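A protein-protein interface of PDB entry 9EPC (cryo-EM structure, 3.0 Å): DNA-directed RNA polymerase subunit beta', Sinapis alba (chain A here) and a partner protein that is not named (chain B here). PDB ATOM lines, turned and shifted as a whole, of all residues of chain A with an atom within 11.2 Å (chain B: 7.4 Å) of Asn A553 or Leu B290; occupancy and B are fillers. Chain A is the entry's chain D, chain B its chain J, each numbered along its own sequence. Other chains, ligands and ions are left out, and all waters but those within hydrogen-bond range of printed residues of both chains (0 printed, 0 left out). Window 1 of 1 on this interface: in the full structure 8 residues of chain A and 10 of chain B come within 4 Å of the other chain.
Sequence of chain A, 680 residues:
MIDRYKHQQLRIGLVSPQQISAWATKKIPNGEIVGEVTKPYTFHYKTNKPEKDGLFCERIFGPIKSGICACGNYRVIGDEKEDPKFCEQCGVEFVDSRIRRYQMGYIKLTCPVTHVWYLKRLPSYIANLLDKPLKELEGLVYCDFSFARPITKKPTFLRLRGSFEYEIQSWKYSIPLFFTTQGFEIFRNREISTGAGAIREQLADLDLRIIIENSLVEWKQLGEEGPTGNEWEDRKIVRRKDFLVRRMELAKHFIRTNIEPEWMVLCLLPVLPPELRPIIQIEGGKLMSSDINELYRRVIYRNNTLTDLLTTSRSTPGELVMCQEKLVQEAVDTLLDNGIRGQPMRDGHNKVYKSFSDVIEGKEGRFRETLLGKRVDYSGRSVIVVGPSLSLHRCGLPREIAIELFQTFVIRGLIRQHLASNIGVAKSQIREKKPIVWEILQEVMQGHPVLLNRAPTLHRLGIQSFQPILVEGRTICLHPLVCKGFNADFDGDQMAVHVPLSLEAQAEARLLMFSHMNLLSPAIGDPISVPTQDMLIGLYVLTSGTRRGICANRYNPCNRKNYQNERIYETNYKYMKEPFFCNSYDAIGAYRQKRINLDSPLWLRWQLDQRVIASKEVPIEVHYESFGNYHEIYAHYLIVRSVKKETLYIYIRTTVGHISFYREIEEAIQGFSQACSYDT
Printed residues of chain B within 4 Å of Arg A547: His B289.
Of the printed residues of chain B, Ile A550 touches Arg B287 and Leu B290.
Of the printed residues of chain B, Cys A551 touches Ala B286 (3.97 Å), His B289 (2.3 Å) and Leu B290 (3.7 Å).
Ala A552 touches one residue of chain B.
Asn A553 touches two residues of chain B.
Of the printed residues of chain B, Arg A554 touches Gln B268 (2.5 Å), Arg B287 (2.6 Å), Leu B290 (3.7 Å), Phe B291 (3.2 Å) and Glu B294 (3.1 Å).
Of chain A, only Ile A550 (3.2 Å), Cys A551 (3.7 Å), Ala A552 (3.3 Å), Asn A553 (3.5 Å) and Arg A554 (3.7 Å) come within 4 Å of Leu B290.
Of chain A, only Arg A554 comes within 4 Å of Phe B291.
Of chain A, only Arg A554 (3.1 Å) comes within 4 Å of Glu B294.
Of the 14 printed residues of chain B, 7 touch a printed residue of chain A.
Hydrophobic or aromatic side chains of chain B within 4 Å of the printed part of chain A: His B289, Leu B290 and Phe B291.
Among the printed residues, Asp or Glu carboxylates within 4 Å of a Lys or Arg side-chain nitrogen of the other chain: Arg A554 with Glu B294 (3.3 Å).
O of Asn A553 lies within hydrogen-bond range of NH1 of Arg B287 (3.4 Å).
The guanidinium group (NH2) of Arg A554 sits at hydrogen-bond distance from the backbone carbonyl oxygen (O) of Gln B268 (2.5 Å).
NH1 of Arg B287 lies within hydrogen-bond range of O of Ile A550 (2.7 Å).
The guanidinium group (NE) of Arg A554 is in salt-bridge range of the side-chain carboxylate (OE1) of Glu B294, 3.3 Å away.
The backbone carbonyl oxygen (O) of Cys A551 sits close to a ring nitrogen (NE2) of His B289 (2.3 Å).
The backbone carbonyl oxygen (O) of Arg A554 lies within hydrogen-bond range of the guanidinium group (NH2) of Arg B287, at 2.6 Å.
NH1 of Arg A547 lies close to ND1 of His B289, 3.4 Å away.
CD1 of Leu B290 touches O of Ile A550, at 3.2 Å.
Cys A551 touches Ala B286.
Cys A551 touches Leu B290.
Leu B290 touches Ala A552 (CD2 to O, 3.3 Å).
Asn A553 touches Leu B290 (O to CD1, 3.5 Å).
N of Arg A554 touches CD1 of Leu B290, at 3.7 Å.
NE of Arg A554 touches CE1 of Phe B291, 3.2 Å away.
OE1 of Gln B268 is in hydrogen-bond range of NE of Arg B295 (3.2 Å).
The guanidinium group of Arg A554 is in hydrogen-bond range of the side-chain hydroxyl of Tyr A555, 3.0 Å away.
O of Phe B291 is in hydrogen-bond range of NE2 of Gln B268 (3.1 Å).
NE2 of Gln B268 sits at hydrogen-bond distance from OE1 of Glu B294, 3.3 Å away.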
ATOM      1  N   THR A 546      22.573   0.946   1.786  1.00  0.00           N
ATOM      2  CA  THR A 546      22.251  -0.307   2.446  1.00  0.00           C
ATOM      3  C   THR A 546      22.814  -1.489   1.672  1.00  0.00           C
ATOM      4  O   THR A 546      22.978  -1.443   0.451  1.00  0.00           O
ATOM      5  CB  THR A 546      20.740  -0.471   2.573  1.00  0.00           C
ATOM      6  OG1 THR A 546      20.209  -0.940   1.329  1.00  0.00           O
ATOM      7  CG2 THR A 546      20.096   0.852   2.899  1.00  0.00           C
ATOM      8  N   ARG A 547      23.122  -2.555   2.402  1.00  0.00           N
ATOM      9  CA  ARG A 547      23.356  -3.839   1.765  1.00  0.00           C
ATOM     10  C   ARG A 547      22.063  -4.314   1.123  1.00  0.00           C
ATOM     11  O   ARG A 547      20.980  -4.170   1.697  1.00  0.00           O
ATOM     12  CB  ARG A 547      23.854  -4.853   2.789  1.00  0.00           C
ATOM     13  CG  ARG A 547      25.054  -4.375   3.580  1.00  0.00           C
ATOM     14  CD  ARG A 547      25.414  -5.362   4.668  1.00  0.00           C
ATOM     15  NE  ARG A 547      26.643  -4.994   5.358  1.00  0.00           N
ATOM     16  CZ  ARG A 547      27.860  -5.287   4.921  1.00  0.00           C
ATOM     17  NH1 ARG A 547      28.048  -5.933   3.782  1.00  0.00           N
ATOM     18  NH2 ARG A 547      28.914  -4.920   5.643  1.00  0.00           N
ATOM     19  N   ARG A 548      22.169  -4.867  -0.078  1.00  0.00           N
ATOM     20  CA  ARG A 548      20.998  -5.190  -0.879  1.00  0.00           C
ATOM     21  C   ARG A 548      20.963  -6.677  -1.192  1.00  0.00           C
ATOM     22  O   ARG A 548      22.005  -7.300  -1.416  1.00  0.00           O
ATOM     23  CB  ARG A 548      20.986  -4.385  -2.180  1.00  0.00           C
ATOM     24  CG  ARG A 548      21.566  -2.991  -2.041  1.00  0.00           C
ATOM     25  CD  ARG A 548      21.129  -2.086  -3.176  1.00  0.00           C
ATOM     26  NE  ARG A 548      19.743  -1.664  -3.022  1.00  0.00           N
ATOM     27  CZ  ARG A 548      19.361  -0.591  -2.345  1.00  0.00           C
ATOM     28  NH1 ARG A 548      20.238   0.198  -1.749  1.00  0.00           N
ATOM     29  NH2 ARG A 548      18.065  -0.302  -2.262  1.00  0.00           N
ATOM     30  N   GLY A 549      19.760  -7.236  -1.198  1.00  0.00           N
ATOM     31  CA  GLY A 549      19.594  -8.610  -1.640  1.00  0.00           C
ATOM     32  C   GLY A 549      20.174  -9.600  -0.653  1.00  0.00           C
ATOM     33  O   GLY A 549      19.956  -9.505   0.559  1.00  0.00           O
ATOM     34  N   ILE A 550      20.926 -10.570  -1.178  1.00  0.00           N
ATOM     35  CA  ILE A 550      21.452 -11.653  -0.358  1.00  0.00           C
ATOM     36  C   ILE A 550      22.457 -11.158   0.665  1.00  0.00           C
ATOM     37  O   ILE A 550      22.783 -11.883   1.610  1.00  0.00           O
ATOM     38  CB  ILE A 550      22.089 -12.737  -1.244  1.00  0.00           C
ATOM     39  CG1 ILE A 550      23.341 -12.188  -1.919  1.00  0.00           C
ATOM     40  CG2 ILE A 550      21.096 -13.224  -2.276  1.00  0.00           C
ATOM     41  CD1 ILE A 550      24.161 -13.238  -2.601  1.00  0.00           C
ATOM     42  N   CYS A 551      22.976  -9.945   0.497  1.00  0.00           N
ATOM     43  CA  CYS A 551      23.895  -9.380   1.473  1.00  0.00           C
ATOM     44  C   CYS A 551      23.178  -8.730   2.645  1.00  0.00           C
ATOM     45  O   CYS A 551      23.842  -8.302   3.593  1.00  0.00           O
ATOM     46  CB  CYS A 551      24.813  -8.359   0.802  1.00  0.00           C
ATOM     47  SG  CYS A 551      25.782  -9.026  -0.565  1.00  0.00           S
ATOM     48  N   ALA A 552      21.852  -8.643   2.605  1.00  0.00           N
ATOM     49  CA  ALA A 552      21.080  -8.036   3.679  1.00  0.00           C
ATOM     50  C   ALA A 552      20.202  -9.019   4.433  1.00  0.00           C
ATOM     51  O   ALA A 552      19.973  -8.827   5.626  1.00  0.00           O
ATOM     52  CB  ALA A 552      20.195  -6.912   3.130  1.00  0.00           C
ATOM     53  N   ASN A 553      19.707 -10.059   3.770  1.00  0.00           N
ATOM     54  CA  ASN A 553      18.855 -11.056   4.399  1.00  0.00           C
ATOM     55  C   ASN A 553      19.455 -12.435   4.195  1.00  0.00           C
ATOM     56  O   ASN A 553      19.922 -12.761   3.102  1.00  0.00           O
ATOM     57  CB  ASN A 553      17.441 -11.016   3.829  1.00  0.00           C
ATOM     58  CG  ASN A 553      16.775  -9.676   4.025  1.00  0.00           C
ATOM     59  OD1 ASN A 553      16.998  -9.003   5.029  1.00  0.00           O
ATOM     60  ND2 ASN A 553      15.952  -9.278   3.066  1.00  0.00           N
ATOM     61  N   ARG A 554      19.445 -13.244   5.256  1.00  0.00           N
ATOM     62  CA  ARG A 554      19.959 -14.602   5.136  1.00  0.00           C
ATOM     63  C   ARG A 554      19.034 -15.467   4.293  1.00  0.00           C
ATOM     64  O   ARG A 554      19.499 -16.314   3.523  1.00  0.00           O
ATOM     65  CB  ARG A 554      20.153 -15.221   6.518  1.00  0.00           C
ATOM     66  CG  ARG A 554      20.974 -16.500   6.509  1.00  0.00           C
ATOM     67  CD  ARG A 554      20.669 -17.349   7.727  1.00  0.00           C
ATOM     68  NE  ARG A 554      21.674 -18.379   7.965  1.00  0.00           N
ATOM     69  CZ  ARG A 554      21.691 -19.564   7.372  1.00  0.00           C
ATOM     70  NH1 ARG A 554      20.787 -19.897   6.468  1.00  0.00           N
ATOM     71  NH2 ARG A 554      22.642 -20.435   7.693  1.00  0.00           N
ATOM     72  N   TYR A 555      17.728 -15.268   4.420  1.00  0.00           N
ATOM     73  CA  TYR A 555      16.742 -16.059   3.705  1.00  0.00           C
ATOM     74  C   TYR A 555      15.931 -15.174   2.772  1.00  0.00           C
ATOM     75  O   TYR A 555      15.810 -13.963   2.974  1.00  0.00           O
ATOM     76  CB  TYR A 555      15.799 -16.784   4.669  1.00  0.00           C
ATOM     77  CG  TYR A 555      16.499 -17.707   5.631  1.00  0.00           C
ATOM     78  CD1 TYR A 555      17.000 -18.926   5.209  1.00  0.00           C
ATOM     79  CD2 TYR A 555      16.652 -17.361   6.963  1.00  0.00           C
ATOM     80  CE1 TYR A 555      17.637 -19.773   6.084  1.00  0.00           C
ATOM     81  CE2 TYR A 555      17.286 -18.203   7.848  1.00  0.00           C
ATOM     82  CZ  TYR A 555      17.779 -19.408   7.403  1.00  0.00           C
ATOM     83  OH  TYR A 555      18.415 -20.251   8.281  1.00  0.00           O
ATOM     84  N   ASN A 556      15.372 -15.798   1.749  1.00  0.00           N
ATOM     85  CA  ASN A 556      14.521 -15.083   0.813  1.00  0.00           C
ATOM     86  C   ASN A 556      13.255 -14.623   1.525  1.00  0.00           C
ATOM     87  O   ASN A 556      12.578 -15.440   2.158  1.00  0.00           O
ATOM     88  CB  ASN A 556      14.171 -15.985  -0.364  1.00  0.00           C
ATOM     89  CG  ASN A 556      13.423 -15.258  -1.455  1.00  0.00           C
ATOM     90  OD1 ASN A 556      13.558 -14.049  -1.615  1.00  0.00           O
ATOM     91  ND2 ASN A 556      12.630 -15.997  -2.218  1.00  0.00           N
ATOM     92  N   PRO A 557      12.910 -13.335   1.464  1.00  0.00           N
ATOM     93  CA  PRO A 557      11.676 -12.881   2.120  1.00  0.00           C
ATOM     94  C   PRO A 557      10.428 -13.578   1.612  1.00  0.00           C
ATOM     95  O   PRO A 557       9.493 -13.788   2.395  1.00  0.00           O
ATOM     96  CB  PRO A 557      11.650 -11.380   1.807  1.00  0.00           C
ATOM     97  CG  PRO A 557      13.074 -11.022   1.603  1.00  0.00           C
ATOM     98  CD  PRO A 557      13.706 -12.210   0.946  1.00  0.00           C
ATOM     99  N   CYS A 558      10.390 -13.939   0.331  1.00  0.00           N
ATOM    100  CA  CYS A 558       9.283 -14.678  -0.281  1.00  0.00           C
ATOM    101  C   CYS A 558       7.913 -14.102   0.064  1.00  0.00           C
ATOM    102  O   CYS A 558       6.882 -14.690  -0.264  1.00  0.00           O
ATOM    103  CB  CYS A 558       9.339 -16.155   0.123  1.00  0.00           C
ATOM    104  SG  CYS A 558       8.511 -16.571   1.680  1.00  0.00           S
ATOM    105  N   GLU A 578      10.992  -1.512   8.694  1.00  0.00           N
ATOM    106  CA  GLU A 578      11.928  -0.397   8.624  1.00  0.00           C
ATOM    107  C   GLU A 578      11.271   0.896   9.088  1.00  0.00           C
ATOM    108  O   GLU A 578      10.101   1.136   8.800  1.00  0.00           O
ATOM    109  CB  GLU A 578      12.468  -0.242   7.205  1.00  0.00           C
ATOM    110  CG  GLU A 578      13.324  -1.408   6.755  1.00  0.00           C
ATOM    111  CD  GLU A 578      13.879  -1.222   5.362  1.00  0.00           C
ATOM    112  OE1 GLU A 578      13.550  -0.203   4.723  1.00  0.00           O
ATOM    113  OE2 GLU A 578      14.642  -2.097   4.904  1.00  0.00           O
ATOM    114  N   ASP A 599      24.173   2.906   7.599  1.00  0.00           N
ATOM    115  CA  ASP A 599      23.753   2.177   6.411  1.00  0.00           C
ATOM    116  C   ASP A 599      22.417   1.471   6.580  1.00  0.00           C
ATOM    117  O   ASP A 599      21.974   0.790   5.653  1.00  0.00           O
ATOM    118  CB  ASP A 599      24.823   1.153   6.022  1.00  0.00           C
ATOM    119  CG  ASP A 599      25.174   0.221   7.163  1.00  0.00           C
ATOM    120  OD1 ASP A 599      25.214   0.688   8.320  1.00  0.00           O
ATOM    121  OD2 ASP A 599      25.405  -0.979   6.904  1.00  0.00           O
ATOM    122  N   SER A 600      21.773   1.606   7.728  1.00  0.00           N
ATOM    123  CA  SER A 600      20.503   0.926   7.949  1.00  0.00           C
ATOM    124  C   SER A 600      19.412   1.573   7.105  1.00  0.00           C
ATOM    125  O   SER A 600      19.293   2.803   7.093  1.00  0.00           O
ATOM    126  CB  SER A 600      20.125   0.968   9.425  1.00  0.00           C
ATOM    127  OG  SER A 600      20.015   2.303   9.877  1.00  0.00           O
ATOM    128  N   PRO A 601      18.605   0.792   6.393  1.00  0.00           N
ATOM    129  CA  PRO A 601      17.569   1.381   5.541  1.00  0.00           C
ATOM    130  C   PRO A 601      16.496   2.073   6.361  1.00  0.00           C
ATOM    131  O   PRO A 601      16.220   1.708   7.505  1.00  0.00           O
ATOM    132  CB  PRO A 601      16.993   0.175   4.789  1.00  0.00           C
ATOM    133  CG  PRO A 601      17.937  -0.955   5.047  1.00  0.00           C
ATOM    134  CD  PRO A 601      18.582  -0.676   6.356  1.00  0.00           C
ATOM    135  N   ARG A 653      13.097   5.508   0.169  1.00  0.00           N
ATOM    136  CA  ARG A 653      13.864   4.495   0.883  1.00  0.00           C
ATOM    137  C   ARG A 653      15.341   4.832   0.733  1.00  0.00           C
ATOM    138  O   ARG A 653      15.909   4.689  -0.352  1.00  0.00           O
ATOM    139  CB  ARG A 653      13.558   3.099   0.352  1.00  0.00           C
ATOM    140  CG  ARG A 653      14.234   1.994   1.139  1.00  0.00           C
ATOM    141  CD  ARG A 653      13.754   0.628   0.697  1.00  0.00           C
ATOM    142  NE  ARG A 653      14.312  -0.436   1.521  1.00  0.00           N
ATOM    143  CZ  ARG A 653      15.440  -1.076   1.252  1.00  0.00           C
ATOM    144  NH1 ARG A 653      16.159  -0.788   0.181  1.00  0.00           N
ATOM    145  NH2 ARG A 653      15.856  -2.031   2.078  1.00  0.00           N
ATOM    146  N   GLN B 268      24.622 -24.055  12.082  1.00  0.00           N
ATOM    147  CA  GLN B 268      24.164 -22.809  11.480  1.00  0.00           C
ATOM    148  C   GLN B 268      24.293 -22.846   9.966  1.00  0.00           C
ATOM    149  O   GLN B 268      23.492 -22.227   9.257  1.00  0.00           O
ATOM    150  CB  GLN B 268      24.953 -21.634  12.055  1.00  0.00           C
ATOM    151  CG  GLN B 268      24.455 -20.273  11.615  1.00  0.00           C
ATOM    152  CD  GLN B 268      25.271 -19.143  12.200  1.00  0.00           C
ATOM    153  OE1 GLN B 268      26.337 -19.364  12.769  1.00  0.00           O
ATOM    154  NE2 GLN B 268      24.771 -17.923  12.067  1.00  0.00           N
ATOM    155  N   TYR B 284      30.996 -17.015   1.674  1.00  0.00           N
ATOM    156  CA  TYR B 284      30.941 -16.638   3.081  1.00  0.00           C
ATOM    157  C   TYR B 284      31.275 -15.165   3.272  1.00  0.00           C
ATOM    158  O   TYR B 284      30.647 -14.486   4.091  1.00  0.00           O
ATOM    159  CB  TYR B 284      31.886 -17.512   3.901  1.00  0.00           C
ATOM    160  CG  TYR B 284      31.984 -17.098   5.348  1.00  0.00           C
ATOM    161  CD1 TYR B 284      30.929 -17.305   6.221  1.00  0.00           C
ATOM    162  CD2 TYR B 284      33.132 -16.501   5.841  1.00  0.00           C
ATOM    163  CE1 TYR B 284      31.015 -16.928   7.543  1.00  0.00           C
ATOM    164  CE2 TYR B 284      33.226 -16.121   7.161  1.00  0.00           C
ATOM    165  CZ  TYR B 284      32.166 -16.337   8.007  1.00  0.00           C
ATOM    166  OH  TYR B 284      32.259 -15.958   9.324  1.00  0.00           O
ATOM    167  N   ARG B 285      32.252 -14.650   2.523  1.00  0.00           N
ATOM    168  CA  ARG B 285      32.623 -13.246   2.665  1.00  0.00           C
ATOM    169  C   ARG B 285      31.453 -12.328   2.340  1.00  0.00           C
ATOM    170  O   ARG B 285      31.266 -11.297   2.994  1.00  0.00           O
ATOM    171  CB  ARG B 285      33.812 -12.915   1.768  1.00  0.00           C
ATOM    172  CG  ARG B 285      35.147 -13.351   2.321  1.00  0.00           C
ATOM    173  CD  ARG B 285      36.283 -12.667   1.590  1.00  0.00           C
ATOM    174  NE  ARG B 285      36.212 -12.889   0.153  1.00  0.00           N
ATOM    175  CZ  ARG B 285      36.769 -13.915  -0.472  1.00  0.00           C
ATOM    176  NH1 ARG B 285      37.450 -14.838   0.186  1.00  0.00           N
ATOM    177  NH2 ARG B 285      36.640 -14.019  -1.791  1.00  0.00           N
ATOM    178  N   ALA B 286      30.661 -12.681   1.329  1.00  0.00           N
ATOM    179  CA  ALA B 286      29.524 -11.848   0.960  1.00  0.00           C
ATOM    180  C   ALA B 286      28.492 -11.792   2.077  1.00  0.00           C
ATOM    181  O   ALA B 286      27.889 -10.742   2.325  1.00  0.00           O
ATOM    182  CB  ALA B 286      28.892 -12.366  -0.330  1.00  0.00           C
ATOM    183  N   ARG B 287      28.276 -12.911   2.765  1.00  0.00           N
ATOM    184  CA  ARG B 287      27.243 -13.021   3.786  1.00  0.00           C
ATOM    185  C   ARG B 287      27.823 -13.227   5.179  1.00  0.00           C
ATOM    186  O   ARG B 287      27.136 -13.742   6.063  1.00  0.00           O
ATOM    187  CB  ARG B 287      26.288 -14.156   3.424  1.00  0.00           C
ATOM    188  CG  ARG B 287      25.675 -13.986   2.051  1.00  0.00           C
ATOM    189  CD  ARG B 287      25.176 -15.296   1.490  1.00  0.00           C
ATOM    190  NE  ARG B 287      24.161 -15.907   2.335  1.00  0.00           N
ATOM    191  CZ  ARG B 287      22.884 -15.553   2.343  1.00  0.00           C
ATOM    192  NH1 ARG B 287      22.440 -14.560   1.594  1.00  0.00           N
ATOM    193  NH2 ARG B 287      22.034 -16.211   3.123  1.00  0.00           N
ATOM    194  N   ARG B 288      29.075 -12.821   5.391  1.00  0.00           N
ATOM    195  CA  ARG B 288      29.724 -13.021   6.682  1.00  0.00           C
ATOM    196  C   ARG B 288      29.012 -12.258   7.790  1.00  0.00           C
ATOM    197  O   ARG B 288      28.852 -12.771   8.903  1.00  0.00           O
ATOM    198  CB  ARG B 288      31.186 -12.593   6.582  1.00  0.00           C
ATOM    199  CG  ARG B 288      31.918 -12.475   7.892  1.00  0.00           C
ATOM    200  CD  ARG B 288      33.328 -11.999   7.624  1.00  0.00           C
ATOM    201  NE  ARG B 288      33.324 -10.855   6.722  1.00  0.00           N
ATOM    202  CZ  ARG B 288      34.382 -10.432   6.044  1.00  0.00           C
ATOM    203  NH1 ARG B 288      35.549 -11.046   6.130  1.00  0.00           N
ATOM    204  NH2 ARG B 288      34.262  -9.368   5.256  1.00  0.00           N
ATOM    205  N   HIS B 289      28.583 -11.029   7.508  1.00  0.00           N
ATOM    206  CA  HIS B 289      27.928 -10.217   8.526  1.00  0.00           C
ATOM    207  C   HIS B 289      26.582 -10.797   8.939  1.00  0.00           C
ATOM    208  O   HIS B 289      26.180 -10.655  10.099  1.00  0.00           O
ATOM    209  CB  HIS B 289      27.748  -8.793   8.012  1.00  0.00           C
ATOM    210  CG  HIS B 289      27.026  -8.721   6.705  1.00  0.00           C
ATOM    211  ND1 HIS B 289      27.666  -8.877   5.495  1.00  0.00           N
ATOM    212  CD2 HIS B 289      25.718  -8.531   6.418  1.00  0.00           C
ATOM    213  CE1 HIS B 289      26.784  -8.778   4.518  1.00  0.00           C
ATOM    214  NE2 HIS B 289      25.593  -8.569   5.051  1.00  0.00           N
ATOM    215  N   LEU B 290      25.868 -11.434   8.010  1.00  0.00           N
ATOM    216  CA  LEU B 290      24.552 -11.978   8.332  1.00  0.00           C
ATOM    217  C   LEU B 290      24.643 -13.058   9.399  1.00  0.00           C
ATOM    218  O   LEU B 290      23.829 -13.094  10.328  1.00  0.00           O
ATOM    219  CB  LEU B 290      23.893 -12.540   7.075  1.00  0.00           C
ATOM    220  CG  LEU B 290      23.618 -11.550   5.951  1.00  0.00           C
ATOM    221  CD1 LEU B 290      22.991 -12.267   4.781  1.00  0.00           C
ATOM    222  CD2 LEU B 290      22.715 -10.443   6.444  1.00  0.00           C
ATOM    223  N   PHE B 291      25.625 -13.952   9.282  1.00  0.00           N
ATOM    224  CA  PHE B 291      25.749 -15.031  10.252  1.00  0.00           C
ATOM    225  C   PHE B 291      26.263 -14.526  11.591  1.00  0.00           C
ATOM    226  O   PHE B 291      25.884 -15.061  12.636  1.00  0.00           O
ATOM    227  CB  PHE B 291      26.661 -16.124   9.705  1.00  0.00           C
ATOM    228  CG  PHE B 291      26.241 -16.636   8.364  1.00  0.00           C
ATOM    229  CD1 PHE B 291      25.000 -17.221   8.194  1.00  0.00           C
ATOM    230  CD2 PHE B 291      27.080 -16.533   7.273  1.00  0.00           C
ATOM    231  CE1 PHE B 291      24.608 -17.691   6.962  1.00  0.00           C
ATOM    232  CE2 PHE B 291      26.691 -17.001   6.039  1.00  0.00           C
ATOM    233  CZ  PHE B 291      25.454 -17.581   5.885  1.00  0.00           C
ATOM    234  N   LYS B 292      27.123 -13.508  11.583  1.00  0.00           N
ATOM    235  CA  LYS B 292      27.589 -12.940  12.843  1.00  0.00           C
ATOM    236  C   LYS B 292      26.439 -12.326  13.625  1.00  0.00           C
ATOM    237  O   LYS B 292      26.364 -12.471  14.850  1.00  0.00           O
ATOM    238  CB  LYS B 292      28.673 -11.896  12.589  1.00  0.00           C
ATOM    239  CG  LYS B 292      29.167 -11.228  13.855  1.00  0.00           C
ATOM    240  CD  LYS B 292      30.133 -10.105  13.556  1.00  0.00           C
ATOM    241  CE  LYS B 292      30.626  -9.465  14.840  1.00  0.00           C
ATOM    242  NZ  LYS B 292      31.599  -8.373  14.575  1.00  0.00           N
ATOM    243  N   GLU B 293      25.532 -11.636  12.933  1.00  0.00           N
ATOM    244  CA  GLU B 293      24.409 -11.002  13.614  1.00  0.00           C
ATOM    245  C   GLU B 293      23.500 -12.041  14.255  1.00  0.00           C
ATOM    246  O   GLU B 293      22.981 -11.826  15.356  1.00  0.00           O
ATOM    247  CB  GLU B 293      23.628 -10.128  12.634  1.00  0.00           C
ATOM    248  CG  GLU B 293      22.894  -8.961  13.279  1.00  0.00           C
ATOM    249  CD  GLU B 293      21.661  -9.386  14.054  1.00  0.00           C
ATOM    250  OE1 GLU B 293      21.047 -10.408  13.683  1.00  0.00           O
ATOM    251  OE2 GLU B 293      21.307  -8.699  15.033  1.00  0.00           O
ATOM    252  N   GLU B 294      23.287 -13.171  13.579  1.00  0.00           N
ATOM    253  CA  GLU B 294      22.447 -14.219  14.148  1.00  0.00           C
ATOM    254  C   GLU B 294      23.042 -14.763  15.439  1.00  0.00           C
ATOM    255  O   GLU B 294      22.316 -15.017  16.405  1.00  0.00           O
ATOM    256  CB  GLU B 294      22.245 -15.343  13.135  1.00  0.00           C
ATOM    257  CG  GLU B 294      21.435 -14.927  11.926  1.00  0.00           C
ATOM    258  CD  GLU B 294      21.035 -16.102  11.061  1.00  0.00           C
ATOM    259  OE1 GLU B 294      21.817 -17.069  10.963  1.00  0.00           O
ATOM    260  OE2 GLU B 294      19.927 -16.059  10.485  1.00  0.00           O
ATOM    261  N   ARG B 295      24.361 -14.958  15.473  1.00  0.00           N
ATOM    262  CA  ARG B 295      25.001 -15.377  16.714  1.00  0.00           C
ATOM    263  C   ARG B 295      24.870 -14.302  17.782  1.00  0.00           C
ATOM    264  O   ARG B 295      24.611 -14.606  18.951  1.00  0.00           O
ATOM    265  CB  ARG B 295      26.472 -15.704  16.471  1.00  0.00           C
ATOM    266  CG  ARG B 295      26.712 -16.666  15.334  1.00  0.00           C
ATOM    267  CD  ARG B 295      28.163 -17.089  15.290  1.00  0.00           C
ATOM    268  NE  ARG B 295      28.577 -17.433  13.938  1.00  0.00           N
ATOM    269  CZ  ARG B 295      29.282 -16.636  13.149  1.00  0.00           C
ATOM    270  NH1 ARG B 295      29.699 -15.452  13.560  1.00  0.00           N
ATOM    271  NH2 ARG B 295      29.580 -17.039  11.919  1.00  0.00           N
ATOM    272  N   LEU B 296      25.052 -13.037  17.399  1.00  0.00           N
ATOM    273  CA  LEU B 296      24.885 -11.946  18.352  1.00  0.00           C
ATOM    274  C   LEU B 296      23.452 -11.875  18.858  1.00  0.00           C
ATOM    275  O   LEU B 296      23.218 -11.639  20.049  1.00  0.00           O
ATOM    276  CB  LEU B 296      25.295 -10.622  17.712  1.00  0.00           C
ATOM    277  CG  LEU B 296      26.798 -10.399  17.575  1.00  0.00           C
ATOM    278  CD1 LEU B 296      27.077  -9.134  16.790  1.00  0.00           C
ATOM    279  CD2 LEU B 296      27.432 -10.326  18.946  1.00  0.00           C
